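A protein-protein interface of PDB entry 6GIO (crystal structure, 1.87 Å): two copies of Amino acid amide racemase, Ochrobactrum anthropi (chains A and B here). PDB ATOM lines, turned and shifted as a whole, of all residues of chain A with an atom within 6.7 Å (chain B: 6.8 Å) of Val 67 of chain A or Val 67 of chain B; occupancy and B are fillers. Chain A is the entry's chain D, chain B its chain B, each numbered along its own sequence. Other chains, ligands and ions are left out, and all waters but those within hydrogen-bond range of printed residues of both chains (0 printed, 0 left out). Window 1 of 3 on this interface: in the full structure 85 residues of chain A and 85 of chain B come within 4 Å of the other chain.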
ATOM      1  N   ALA A  62      18.501 -29.192 -10.204  1.00  0.00           N
ATOM      2  CA  ALA A  62      17.741 -30.425 -10.494  1.00  0.00           C
ATOM      3  C   ALA A  62      16.371 -30.410  -9.812  1.00  0.00           C
ATOM      4  O   ALA A  62      15.365 -30.787 -10.418  1.00  0.00           O
ATOM      5  CB  ALA A  62      18.519 -31.666 -10.091  1.00  0.00           C
ATOM      6  N   ILE A  63      16.338 -29.957  -8.557  1.00  0.00           N
ATOM      7  CA  ILE A  63      15.072 -29.805  -7.823  1.00  0.00           C
ATOM      8  C   ILE A  63      14.248 -28.665  -8.425  1.00  0.00           C
ATOM      9  O   ILE A  63      13.049 -28.804  -8.599  1.00  0.00           O
ATOM     10  CB  ILE A  63      15.324 -29.560  -6.310  1.00  0.00           C
ATOM     11  CG1 ILE A  63      15.886 -30.849  -5.653  1.00  0.00           C
ATOM     12  CG2 ILE A  63      14.068 -29.089  -5.583  1.00  0.00           C
ATOM     13  CD1 ILE A  63      16.666 -30.620  -4.372  1.00  0.00           C
ATOM     14  N   VAL A  64      14.879 -27.534  -8.723  1.00  0.00           N
ATOM     15  CA  VAL A  64      14.182 -26.397  -9.333  1.00  0.00           C
ATOM     16  C   VAL A  64      13.526 -26.810 -10.657  1.00  0.00           C
ATOM     17  O   VAL A  64      12.315 -26.567 -10.874  1.00  0.00           O
ATOM     18  CB  VAL A  64      15.107 -25.149  -9.496  1.00  0.00           C
ATOM     19  CG1 VAL A  64      14.423 -24.053 -10.304  1.00  0.00           C
ATOM     20  CG2 VAL A  64      15.480 -24.552  -8.131  1.00  0.00           C
ATOM     21  N   GLU A  65      14.279 -27.454 -11.543  1.00  0.00           N
ATOM     22  CA  GLU A  65      13.688 -27.863 -12.839  1.00  0.00           C
ATOM     23  C   GLU A  65      12.500 -28.790 -12.643  1.00  0.00           C
ATOM     24  O   GLU A  65      11.473 -28.587 -13.239  1.00  0.00           O
ATOM     25  CB  GLU A  65      14.700 -28.551 -13.771  1.00  0.00           C
ATOM     26  N   ALA A  66      12.644 -29.779 -11.776  1.00  0.00           N
ATOM     27  CA  ALA A  66      11.595 -30.775 -11.521  1.00  0.00           C
ATOM     28  C   ALA A  66      10.347 -30.126 -10.981  1.00  0.00           C
ATOM     29  O   ALA A  66       9.252 -30.485 -11.414  1.00  0.00           O
ATOM     30  CB  ALA A  66      12.079 -31.833 -10.550  1.00  0.00           C
ATOM     31  N   VAL A  67      10.517 -29.161 -10.059  1.00  0.00           N
ATOM     32  CA  VAL A  67       9.385 -28.512  -9.425  1.00  0.00           C
ATOM     33  C   VAL A  67       8.714 -27.515 -10.397  1.00  0.00           C
ATOM     34  O   VAL A  67       7.484 -27.414 -10.460  1.00  0.00           O
ATOM     35  CB  VAL A  67       9.817 -27.844  -8.090  1.00  0.00           C
ATOM     36  CG1 VAL A  67       8.783 -26.848  -7.584  1.00  0.00           C
ATOM     37  CG2 VAL A  67      10.080 -28.916  -7.044  1.00  0.00           C
ATOM     38  N   GLU A  68       9.521 -26.794 -11.160  1.00  0.00           N
ATOM     39  CA  GLU A  68       9.021 -25.906 -12.246  1.00  0.00           C
ATOM     40  C   GLU A  68       8.149 -26.655 -13.262  1.00  0.00           C
ATOM     41  O   GLU A  68       7.019 -26.257 -13.532  1.00  0.00           O
ATOM     42  CB  GLU A  68      10.214 -25.279 -12.989  1.00  0.00           C
ATOM     43  CG  GLU A  68      10.829 -24.071 -12.284  1.00  0.00           C
ATOM     44  CD  GLU A  68      12.047 -23.506 -13.026  1.00  0.00           C
ATOM     45  OE1 GLU A  68      12.694 -24.257 -13.831  1.00  0.00           O
ATOM     46  OE2 GLU A  68      12.359 -22.317 -12.768  1.00  0.00           O
ATOM     47  N   LYS A  69       8.699 -27.734 -13.825  1.00  0.00           N
ATOM     48  CA  LYS A  69       8.008 -28.513 -14.842  1.00  0.00           C
ATOM     49  C   LYS A  69       6.686 -29.029 -14.296  1.00  0.00           C
ATOM     50  O   LYS A  69       5.672 -28.921 -14.942  1.00  0.00           O
ATOM     51  CB  LYS A  69       8.901 -29.675 -15.282  1.00  0.00           C
ATOM     52  CG  LYS A  69       8.352 -30.546 -16.407  1.00  0.00           C
ATOM     53  N   SER A  70       6.684 -29.536 -13.065  1.00  0.00           N
ATOM     54  CA  SER A  70       5.484 -30.145 -12.539  1.00  0.00           C
ATOM     55  C   SER A  70       4.385 -29.109 -12.192  1.00  0.00           C
ATOM     56  O   SER A  70       3.221 -29.289 -12.572  1.00  0.00           O
ATOM     57  CB  SER A  70       5.838 -31.027 -11.339  1.00  0.00           C
ATOM     58  OG  SER A  70       4.652 -31.544 -10.845  1.00  0.00           O
ATOM     59  N   VAL A  71       4.727 -28.009 -11.510  1.00  0.00           N
ATOM     60  CA  VAL A  71       3.693 -27.060 -11.106  1.00  0.00           C
ATOM     61  C   VAL A  71       3.024 -26.322 -12.296  1.00  0.00           C
ATOM     62  O   VAL A  71       1.894 -25.824 -12.189  1.00  0.00           O
ATOM     63  CB  VAL A  71       4.276 -26.032 -10.123  1.00  0.00           C
ATOM     64  CG1 VAL A  71       5.230 -25.070 -10.822  1.00  0.00           C
ATOM     65  CG2 VAL A  71       3.167 -25.272  -9.408  1.00  0.00           C
ATOM     66  N   ARG A  72       3.739 -26.239 -13.423  1.00  0.00           N
ATOM     67  CA  ARG A  72       3.230 -25.604 -14.633  1.00  0.00           C
ATOM     68  C   ARG A  72       2.318 -26.539 -15.423  1.00  0.00           C
ATOM     69  O   ARG A  72       1.424 -26.087 -16.111  1.00  0.00           O
ATOM     70  CB  ARG A  72       4.376 -25.187 -15.565  1.00  0.00           C
ATOM     71  CG  ARG A  72       5.298 -24.103 -15.056  1.00  0.00           C
ATOM     72  CD  ARG A  72       6.593 -24.073 -15.886  1.00  0.00           C
ATOM     73  NE  ARG A  72       7.554 -23.143 -15.293  1.00  0.00           N
ATOM     74  CZ  ARG A  72       8.872 -23.170 -15.479  1.00  0.00           C
ATOM     75  NH1 ARG A  72       9.444 -24.091 -16.276  1.00  0.00           N
ATOM     76  NH2 ARG A  72       9.632 -22.260 -14.856  1.00  0.00           N
ATOM     77  N   GLY A 270      12.439 -35.333   0.055  1.00  0.00           N
ATOM     78  CA  GLY A 270      11.749 -34.239  -0.600  1.00  0.00           C
ATOM     79  C   GLY A 270      12.624 -33.135  -1.178  1.00  0.00           C
ATOM     80  O   GLY A 270      12.123 -32.263  -1.889  1.00  0.00           O
ATOM     81  N   LEU A 273      11.050 -30.106  -0.166  1.00  0.00           N
ATOM     82  CA  LEU A 273       9.554 -30.232  -0.263  1.00  0.00           C
ATOM     83  C   LEU A 273       9.042 -31.346   0.674  1.00  0.00           C
ATOM     84  O   LEU A 273       9.780 -32.288   0.962  1.00  0.00           O
ATOM     85  CB  LEU A 273       9.088 -30.494  -1.704  1.00  0.00           C
ATOM     86  CG  LEU A 273       9.015 -29.207  -2.540  1.00  0.00           C
ATOM     87  CD1 LEU A 273      10.343 -28.836  -3.163  1.00  0.00           C
ATOM     88  CD2 LEU A 273       8.019 -29.337  -3.647  1.00  0.00           C
ATOM     89  N   PRO A 300       2.136 -34.665  -7.652  1.00  0.00           N
ATOM     90  CA  PRO A 300       3.225 -34.684  -8.662  1.00  0.00           C
ATOM     91  C   PRO A 300       4.351 -33.642  -8.449  1.00  0.00           C
ATOM     92  O   PRO A 300       5.355 -33.752  -9.089  1.00  0.00           O
ATOM     93  CB  PRO A 300       2.483 -34.400  -9.964  1.00  0.00           C
ATOM     94  CG  PRO A 300       1.265 -33.660  -9.546  1.00  0.00           C
ATOM     95  CD  PRO A 300       0.855 -34.251  -8.228  1.00  0.00           C
ATOM     96  N   VAL A 301       4.176 -32.642  -7.573  1.00  0.00           N
ATOM     97  CA  VAL A 301       5.199 -31.630  -7.366  1.00  0.00           C
ATOM     98  C   VAL A 301       6.267 -32.164  -6.391  1.00  0.00           C
ATOM     99  O   VAL A 301       7.478 -32.199  -6.715  1.00  0.00           O
ATOM    100  CB  VAL A 301       4.579 -30.299  -6.842  1.00  0.00           C
ATOM    101  CG1 VAL A 301       5.665 -29.236  -6.617  1.00  0.00           C
ATOM    102  CG2 VAL A 301       3.547 -29.795  -7.835  1.00  0.00           C
ATOM    103  N   ALA A 302       5.832 -32.598  -5.195  1.00  0.00           N
ATOM    104  CA  ALA A 302       6.751 -33.177  -4.205  1.00  0.00           C
ATOM    105  C   ALA A 302       7.422 -34.431  -4.731  1.00  0.00           C
ATOM    106  O   ALA A 302       8.588 -34.590  -4.534  1.00  0.00           O
ATOM    107  CB  ALA A 302       6.037 -33.479  -2.925  1.00  0.00           C
ATOM    108  N   ALA A 304       8.058 -35.317  -7.898  1.00  0.00           N
ATOM    109  CA  ALA A 304       8.989 -34.913  -8.927  1.00  0.00           C
ATOM    110  C   ALA A 304      10.244 -34.415  -8.277  1.00  0.00           C
ATOM    111  O   ALA A 304      11.330 -34.691  -8.775  1.00  0.00           O
ATOM    112  CB  ALA A 304       8.363 -33.813  -9.806  1.00  0.00           C
ATOM    113  N   ALA A 305      10.110 -33.662  -7.158  1.00  0.00           N
ATOM    114  CA  ALA A 305      11.279 -33.192  -6.437  1.00  0.00           C
ATOM    115  C   ALA A 305      12.089 -34.385  -5.882  1.00  0.00           C
ATOM    116  O   ALA A 305      13.328 -34.389  -5.883  1.00  0.00           O
ATOM    117  CB  ALA A 305      10.865 -32.202  -5.306  1.00  0.00           C
ATOM    118  N   ALA A 308      14.269 -36.064  -8.487  1.00  0.00           N
ATOM    119  CA  ALA A 308      15.482 -35.292  -8.772  1.00  0.00           C
ATOM    120  C   ALA A 308      16.542 -35.479  -7.693  1.00  0.00           C
ATOM    121  O   ALA A 308      17.761 -35.525  -7.977  1.00  0.00           O
ATOM    122  CB  ALA A 308      15.143 -33.814  -8.915  1.00  0.00           C
ATOM    123  N   ALA B  62      -0.678 -17.554 -10.782  1.00  0.00           N
ATOM    124  CA  ALA B  62      -0.314 -17.008  -9.461  1.00  0.00           C
ATOM    125  C   ALA B  62       0.437 -18.077  -8.653  1.00  0.00           C
ATOM    126  O   ALA B  62       1.412 -17.797  -7.953  1.00  0.00           O
ATOM    127  CB  ALA B  62      -1.546 -16.528  -8.701  1.00  0.00           C
ATOM    128  N   ILE B  63      -0.023 -19.315  -8.757  1.00  0.00           N
ATOM    129  CA  ILE B  63       0.570 -20.396  -7.975  1.00  0.00           C
ATOM    130  C   ILE B  63       1.895 -20.776  -8.605  1.00  0.00           C
ATOM    131  O   ILE B  63       2.897 -20.948  -7.888  1.00  0.00           O
ATOM    132  CB  ILE B  63      -0.368 -21.604  -7.864  1.00  0.00           C
ATOM    133  CG1 ILE B  63      -1.573 -21.192  -7.004  1.00  0.00           C
ATOM    134  CG2 ILE B  63       0.360 -22.787  -7.258  1.00  0.00           C
ATOM    135  CD1 ILE B  63      -2.670 -22.210  -7.054  1.00  0.00           C
ATOM    136  N   VAL B  64       1.913 -20.867  -9.937  1.00  0.00           N
ATOM    137  CA  VAL B  64       3.159 -21.130 -10.662  1.00  0.00           C
ATOM    138  C   VAL B  64       4.244 -20.096 -10.250  1.00  0.00           C
ATOM    139  O   VAL B  64       5.340 -20.475  -9.822  1.00  0.00           O
ATOM    140  CB  VAL B  64       2.943 -21.121 -12.184  1.00  0.00           C
ATOM    141  CG1 VAL B  64       4.263 -21.056 -12.912  1.00  0.00           C
ATOM    142  CG2 VAL B  64       2.196 -22.365 -12.609  1.00  0.00           C
ATOM    143  N   GLU B  65       3.924 -18.812 -10.341  1.00  0.00           N
ATOM    144  CA  GLU B  65       4.872 -17.769  -9.926  1.00  0.00           C
ATOM    145  C   GLU B  65       5.364 -17.934  -8.479  1.00  0.00           C
ATOM    146  O   GLU B  65       6.552 -17.840  -8.249  1.00  0.00           O
ATOM    147  CB  GLU B  65       4.310 -16.354 -10.130  1.00  0.00           C
ATOM    148  N   ALA B  66       4.475 -18.121  -7.504  1.00  0.00           N
ATOM    149  CA  ALA B  66       4.899 -18.236  -6.094  1.00  0.00           C
ATOM    150  C   ALA B  66       5.816 -19.434  -5.880  1.00  0.00           C
ATOM    151  O   ALA B  66       6.807 -19.339  -5.180  1.00  0.00           O
ATOM    152  CB  ALA B  66       3.686 -18.324  -5.158  1.00  0.00           C
ATOM    153  N   VAL B  67       5.476 -20.552  -6.519  1.00  0.00           N
ATOM    154  CA  VAL B  67       6.259 -21.773  -6.421  1.00  0.00           C
ATOM    155  C   VAL B  67       7.637 -21.595  -7.082  1.00  0.00           C
ATOM    156  O   VAL B  67       8.675 -21.984  -6.504  1.00  0.00           O
ATOM    157  CB  VAL B  67       5.439 -22.989  -6.967  1.00  0.00           C
ATOM    158  CG1 VAL B  67       6.279 -24.241  -7.134  1.00  0.00           C
ATOM    159  CG2 VAL B  67       4.281 -23.282  -6.024  1.00  0.00           C
ATOM    160  N   GLU B  68       7.672 -20.969  -8.260  1.00  0.00           N
ATOM    161  CA  GLU B  68       8.954 -20.749  -8.948  1.00  0.00           C
ATOM    162  C   GLU B  68       9.887 -19.874  -8.130  1.00  0.00           C
ATOM    163  O   GLU B  68      11.046 -20.230  -7.937  1.00  0.00           O
ATOM    164  CB  GLU B  68       8.754 -20.077 -10.278  1.00  0.00           C
ATOM    165  CG  GLU B  68       8.284 -21.034 -11.337  1.00  0.00           C
ATOM    166  CD  GLU B  68       7.920 -20.298 -12.610  1.00  0.00           C
ATOM    167  OE1 GLU B  68       7.546 -19.080 -12.540  1.00  0.00           O
ATOM    168  OE2 GLU B  68       8.035 -20.956 -13.664  1.00  0.00           O
ATOM    169  N   LYS B  69       9.379 -18.750  -7.635  1.00  0.00           N
ATOM    170  CA  LYS B  69      10.227 -17.841  -6.851  1.00  0.00           C
ATOM    171  C   LYS B  69      10.782 -18.525  -5.600  1.00  0.00           C
ATOM    172  O   LYS B  69      11.986 -18.431  -5.324  1.00  0.00           O
ATOM    173  CB  LYS B  69       9.496 -16.535  -6.526  1.00  0.00           C
ATOM    174  CG  LYS B  69       9.307 -15.644  -7.769  1.00  0.00           C
ATOM    175  CD  LYS B  69       8.274 -14.527  -7.605  1.00  0.00           C
ATOM    176  CE  LYS B  69       8.377 -13.821  -6.270  1.00  0.00           C
ATOM    177  NZ  LYS B  69       7.403 -12.689  -6.207  1.00  0.00           N
ATOM    178  N   SER B  70       9.934 -19.262  -4.879  1.00  0.00           N
ATOM    179  CA  SER B  70      10.371 -19.962  -3.652  1.00  0.00           C
ATOM    180  C   SER B  70      11.303 -21.139  -3.843  1.00  0.00           C
ATOM    181  O   SER B  70      12.246 -21.298  -3.082  1.00  0.00           O
ATOM    182  CB  SER B  70       9.152 -20.376  -2.773  1.00  0.00           C
ATOM    183  OG  SER B  70       8.159 -21.077  -3.552  1.00  0.00           O
ATOM    184  N   VAL B  71      11.066 -21.992  -4.834  1.00  0.00           N
ATOM    185  CA  VAL B  71      11.954 -23.142  -5.034  1.00  0.00           C
ATOM    186  C   VAL B  71      13.332 -22.697  -5.565  1.00  0.00           C
ATOM    187  O   VAL B  71      14.353 -23.293  -5.231  1.00  0.00           O
ATOM    188  CB  VAL B  71      11.304 -24.196  -5.953  1.00  0.00           C
ATOM    189  CG1 VAL B  71      11.283 -23.737  -7.399  1.00  0.00           C
ATOM    190  CG2 VAL B  71      12.002 -25.533  -5.826  1.00  0.00           C
ATOM    191  N   ARG B  72      13.371 -21.638  -6.382  1.00  0.00           N
ATOM    192  CA  ARG B  72      14.637 -21.032  -6.815  1.00  0.00           C
ATOM    193  C   ARG B  72      15.452 -20.334  -5.719  1.00  0.00           C
ATOM    194  O   ARG B  72      16.681 -20.320  -5.754  1.00  0.00           O
ATOM    195  CB  ARG B  72      14.360 -19.995  -7.906  1.00  0.00           C
ATOM    196  CG  ARG B  72      13.891 -20.577  -9.221  1.00  0.00           C
ATOM    197  CD  ARG B  72      13.248 -19.469 -10.039  1.00  0.00           C
ATOM    198  NE  ARG B  72      12.642 -19.969 -11.265  1.00  0.00           N
ATOM    199  CZ  ARG B  72      11.987 -19.206 -12.137  1.00  0.00           C
ATOM    200  NH1 ARG B  72      11.876 -17.902 -11.935  1.00  0.00           N
ATOM    201  NH2 ARG B  72      11.479 -19.745 -13.222  1.00  0.00           N
ATOM    202  N   ASP B  73      14.772 -19.694  -4.776  1.00  0.00           N
ATOM    203  CA  ASP B  73      15.439 -18.923  -3.760  1.00  0.00           C
ATOM    204  C   ASP B  73      14.758 -19.262  -2.425  1.00  0.00           C
ATOM    205  O   ASP B  73      13.930 -18.511  -1.910  1.00  0.00           O
ATOM    206  CB  ASP B  73      15.376 -17.452  -4.134  1.00  0.00           C
ATOM    207  CG  ASP B  73      16.086 -16.551  -3.141  1.00  0.00           C
ATOM    208  OD1 ASP B  73      16.833 -17.060  -2.303  1.00  0.00           O
ATOM    209  OD2 ASP B  73      15.893 -15.332  -3.194  1.00  0.00           O
ATOM    210  N   GLY B 270      -3.548 -24.984  -0.097  1.00  0.00           N
ATOM    211  CA  GLY B 270      -2.267 -25.173  -0.741  1.00  0.00           C
ATOM    212  C   GLY B 270      -2.274 -25.076  -2.264  1.00  0.00           C
ATOM    213  O   GLY B 270      -1.208 -25.071  -2.884  1.00  0.00           O
ATOM    214  N   LEU B 273      -0.378 -27.927  -3.591  1.00  0.00           N
ATOM    215  CA  LEU B 273       0.752 -28.288  -2.748  1.00  0.00           C
ATOM    216  C   LEU B 273       0.222 -28.621  -1.359  1.00  0.00           C
ATOM    217  O   LEU B 273      -0.813 -28.088  -0.949  1.00  0.00           O
ATOM    218  CB  LEU B 273       1.796 -27.173  -2.667  1.00  0.00           C
ATOM    219  CG  LEU B 273       2.744 -27.069  -3.871  1.00  0.00           C
ATOM    220  CD1 LEU B 273       2.055 -26.360  -5.016  1.00  0.00           C
ATOM    221  CD2 LEU B 273       4.000 -26.315  -3.483  1.00  0.00           C
ATOM    222  N   VAL B 301       7.910 -22.903   0.283  1.00  0.00           N
ATOM    223  CA  VAL B 301       7.293 -23.221  -1.008  1.00  0.00           C
ATOM    224  C   VAL B 301       5.779 -23.404  -0.886  1.00  0.00           C
ATOM    225  O   VAL B 301       5.010 -22.754  -1.595  1.00  0.00           O
ATOM    226  CB  VAL B 301       7.946 -24.466  -1.617  1.00  0.00           C
ATOM    227  CG1 VAL B 301       7.290 -24.822  -2.934  1.00  0.00           C
ATOM    228  CG2 VAL B 301       9.446 -24.204  -1.821  1.00  0.00           C
ATOM    229  N   ALA B 302       5.348 -24.257   0.049  1.00  0.00           N
ATOM    230  CA  ALA B 302       3.957 -24.542   0.258  1.00  0.00           C
ATOM    231  C   ALA B 302       3.282 -23.295   0.754  1.00  0.00           C
ATOM    232  O   ALA B 302       2.187 -23.006   0.284  1.00  0.00           O
ATOM    233  CB  ALA B 302       3.793 -25.670   1.273  1.00  0.00           C
ATOM    234  N   ALA B 304       4.173 -20.098   0.294  1.00  0.00           N
ATOM    235  CA  ALA B 304       4.054 -19.164  -0.816  1.00  0.00           C
ATOM    236  C   ALA B 304       2.837 -19.524  -1.715  1.00  0.00           C
ATOM    237  O   ALA B 304       2.079 -18.631  -2.114  1.00  0.00           O
ATOM    238  CB  ALA B 304       5.347 -19.076  -1.636  1.00  0.00           C
ATOM    239  N   ALA B 305       2.652 -20.818  -2.037  1.00  0.00           N
ATOM    240  CA  ALA B 305       1.493 -21.235  -2.824  1.00  0.00           C
ATOM    241  C   ALA B 305       0.183 -20.815  -2.123  1.00  0.00           C
ATOM    242  O   ALA B 305      -0.762 -20.338  -2.742  1.00  0.00           O
ATOM    243  CB  ALA B 305       1.529 -22.735  -3.088  1.00  0.00           C
ATOM    244  N   ALA B 308      -0.624 -17.177  -2.598  1.00  0.00           N
ATOM    245  CA  ALA B 308      -1.147 -16.968  -3.937  1.00  0.00           C
ATOM    246  C   ALA B 308      -2.603 -17.399  -4.002  1.00  0.00           C
ATOM    247  O   ALA B 308      -3.439 -16.744  -4.633  1.00  0.00           O
ATOM    248  CB  ALA B 308      -0.320 -17.722  -4.983  1.00  0.00           C
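Printed residues of chain A that touch a printed residue of chain B: Val 64, Val 67, Glu 68, Val 71 and Arg 72.
Along chain A the printed residues that touch a printed residue of chain B span positions 64 to 72.
Of the 19 printed residues of chain B, 5 touch a printed residue of chain A.
Among the printed residues, 10 pairs touch across the chains.
Among the printed residues, Asp or Glu carboxylates within 4 Å of a Lys or Arg side-chain nitrogen of the other chain: Glu 68 of chain A with Arg 72 of chain B and Arg 72 of chain A with Glu 68 of chain B.
The guanidinium group of Arg 72 of chain A is in salt-bridge range of the side-chain carboxylate of Glu 68 of chain A, 3.4 Å away.
The side-chain carboxylate of Glu 68 of chain B is in salt-bridge range of the guanidinium group of Arg 72 of chain B (3.7 Å).
O of Val 67 of chain B sits at hydrogen-bond distance from OG of Ser 70 of chain B (3.1 Å).
O of Val 71 of chain B touches CG2 of Val 64 of chain A, 3.4 Å away.
Val 64 of chain A touches Arg 72 of chain B.
Val 67 of chain A touches Val 67 of chain B.
Val 67 of chain A touches Val 71 of chain B.
O of Val 71 of chain A touches CG2 of Val 64 of chain B (3.5 Å).
Val 67 of chain B touches Val 71 of chain A.
Val 64 of chain B touches Arg 72 of chain A.
Arg 72 of chain B touches Arg 72 of chain A.
Val 64 of chain A touches Arg 72 of chain B, and with the chains exchanged Arg 72 of chain A touches Val 64 of chain B.
Val 67 of chain A touches its own counterpart, Val 67 of chain B.
Val 67 of chain A touches Val 71 of chain B, and with the chains exchanged Val 71 of chain A touches Val 67 of chain B.
Arg 72 of chain B touches its own counterpart, Arg 72 of chain A.
OE2 of Glu 68 of chain A is in salt-bridge range of NH2 of Arg 72 of chain B, 2.8 Å away.
The guanidinium group of Arg 72 of chain A lies within salt-bridge range of the side-chain carboxylate of Glu 68 of chain B (2.8 Å).
Val 67 of chain A touches just these residues of chain B: Val 67 (3.6 Å) and Val 71 (3.9 Å).
Of chain A, only Val 67 (3.6 Å) and Val 71 (3.9 Å) come within 4 Å of Val 67 of chain B.
Of the printed residues of chain A, Val 64 of chain B touches Val 71 and Arg 72.
Printed residues of chain B within 4 Å of Val 64 of chain A: Val 71 and Arg 72.
Of the printed residues of chain B, Glu 68 of chain A touches Arg 72 (2.8 Å).
Of the printed residues of chain B, Val 71 of chain A touches Val 64 and Val 67.
Lys 69 of chain A touches none of the printed residues of chain B.
The nearest residue of chain B that does not touch Val 67 of chain A is Val 301 of chain B (5.3 Å).
The nearest printed residue of chain A that does not touch Arg 72 of chain B is Val 67 of chain A (7.0 Å).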
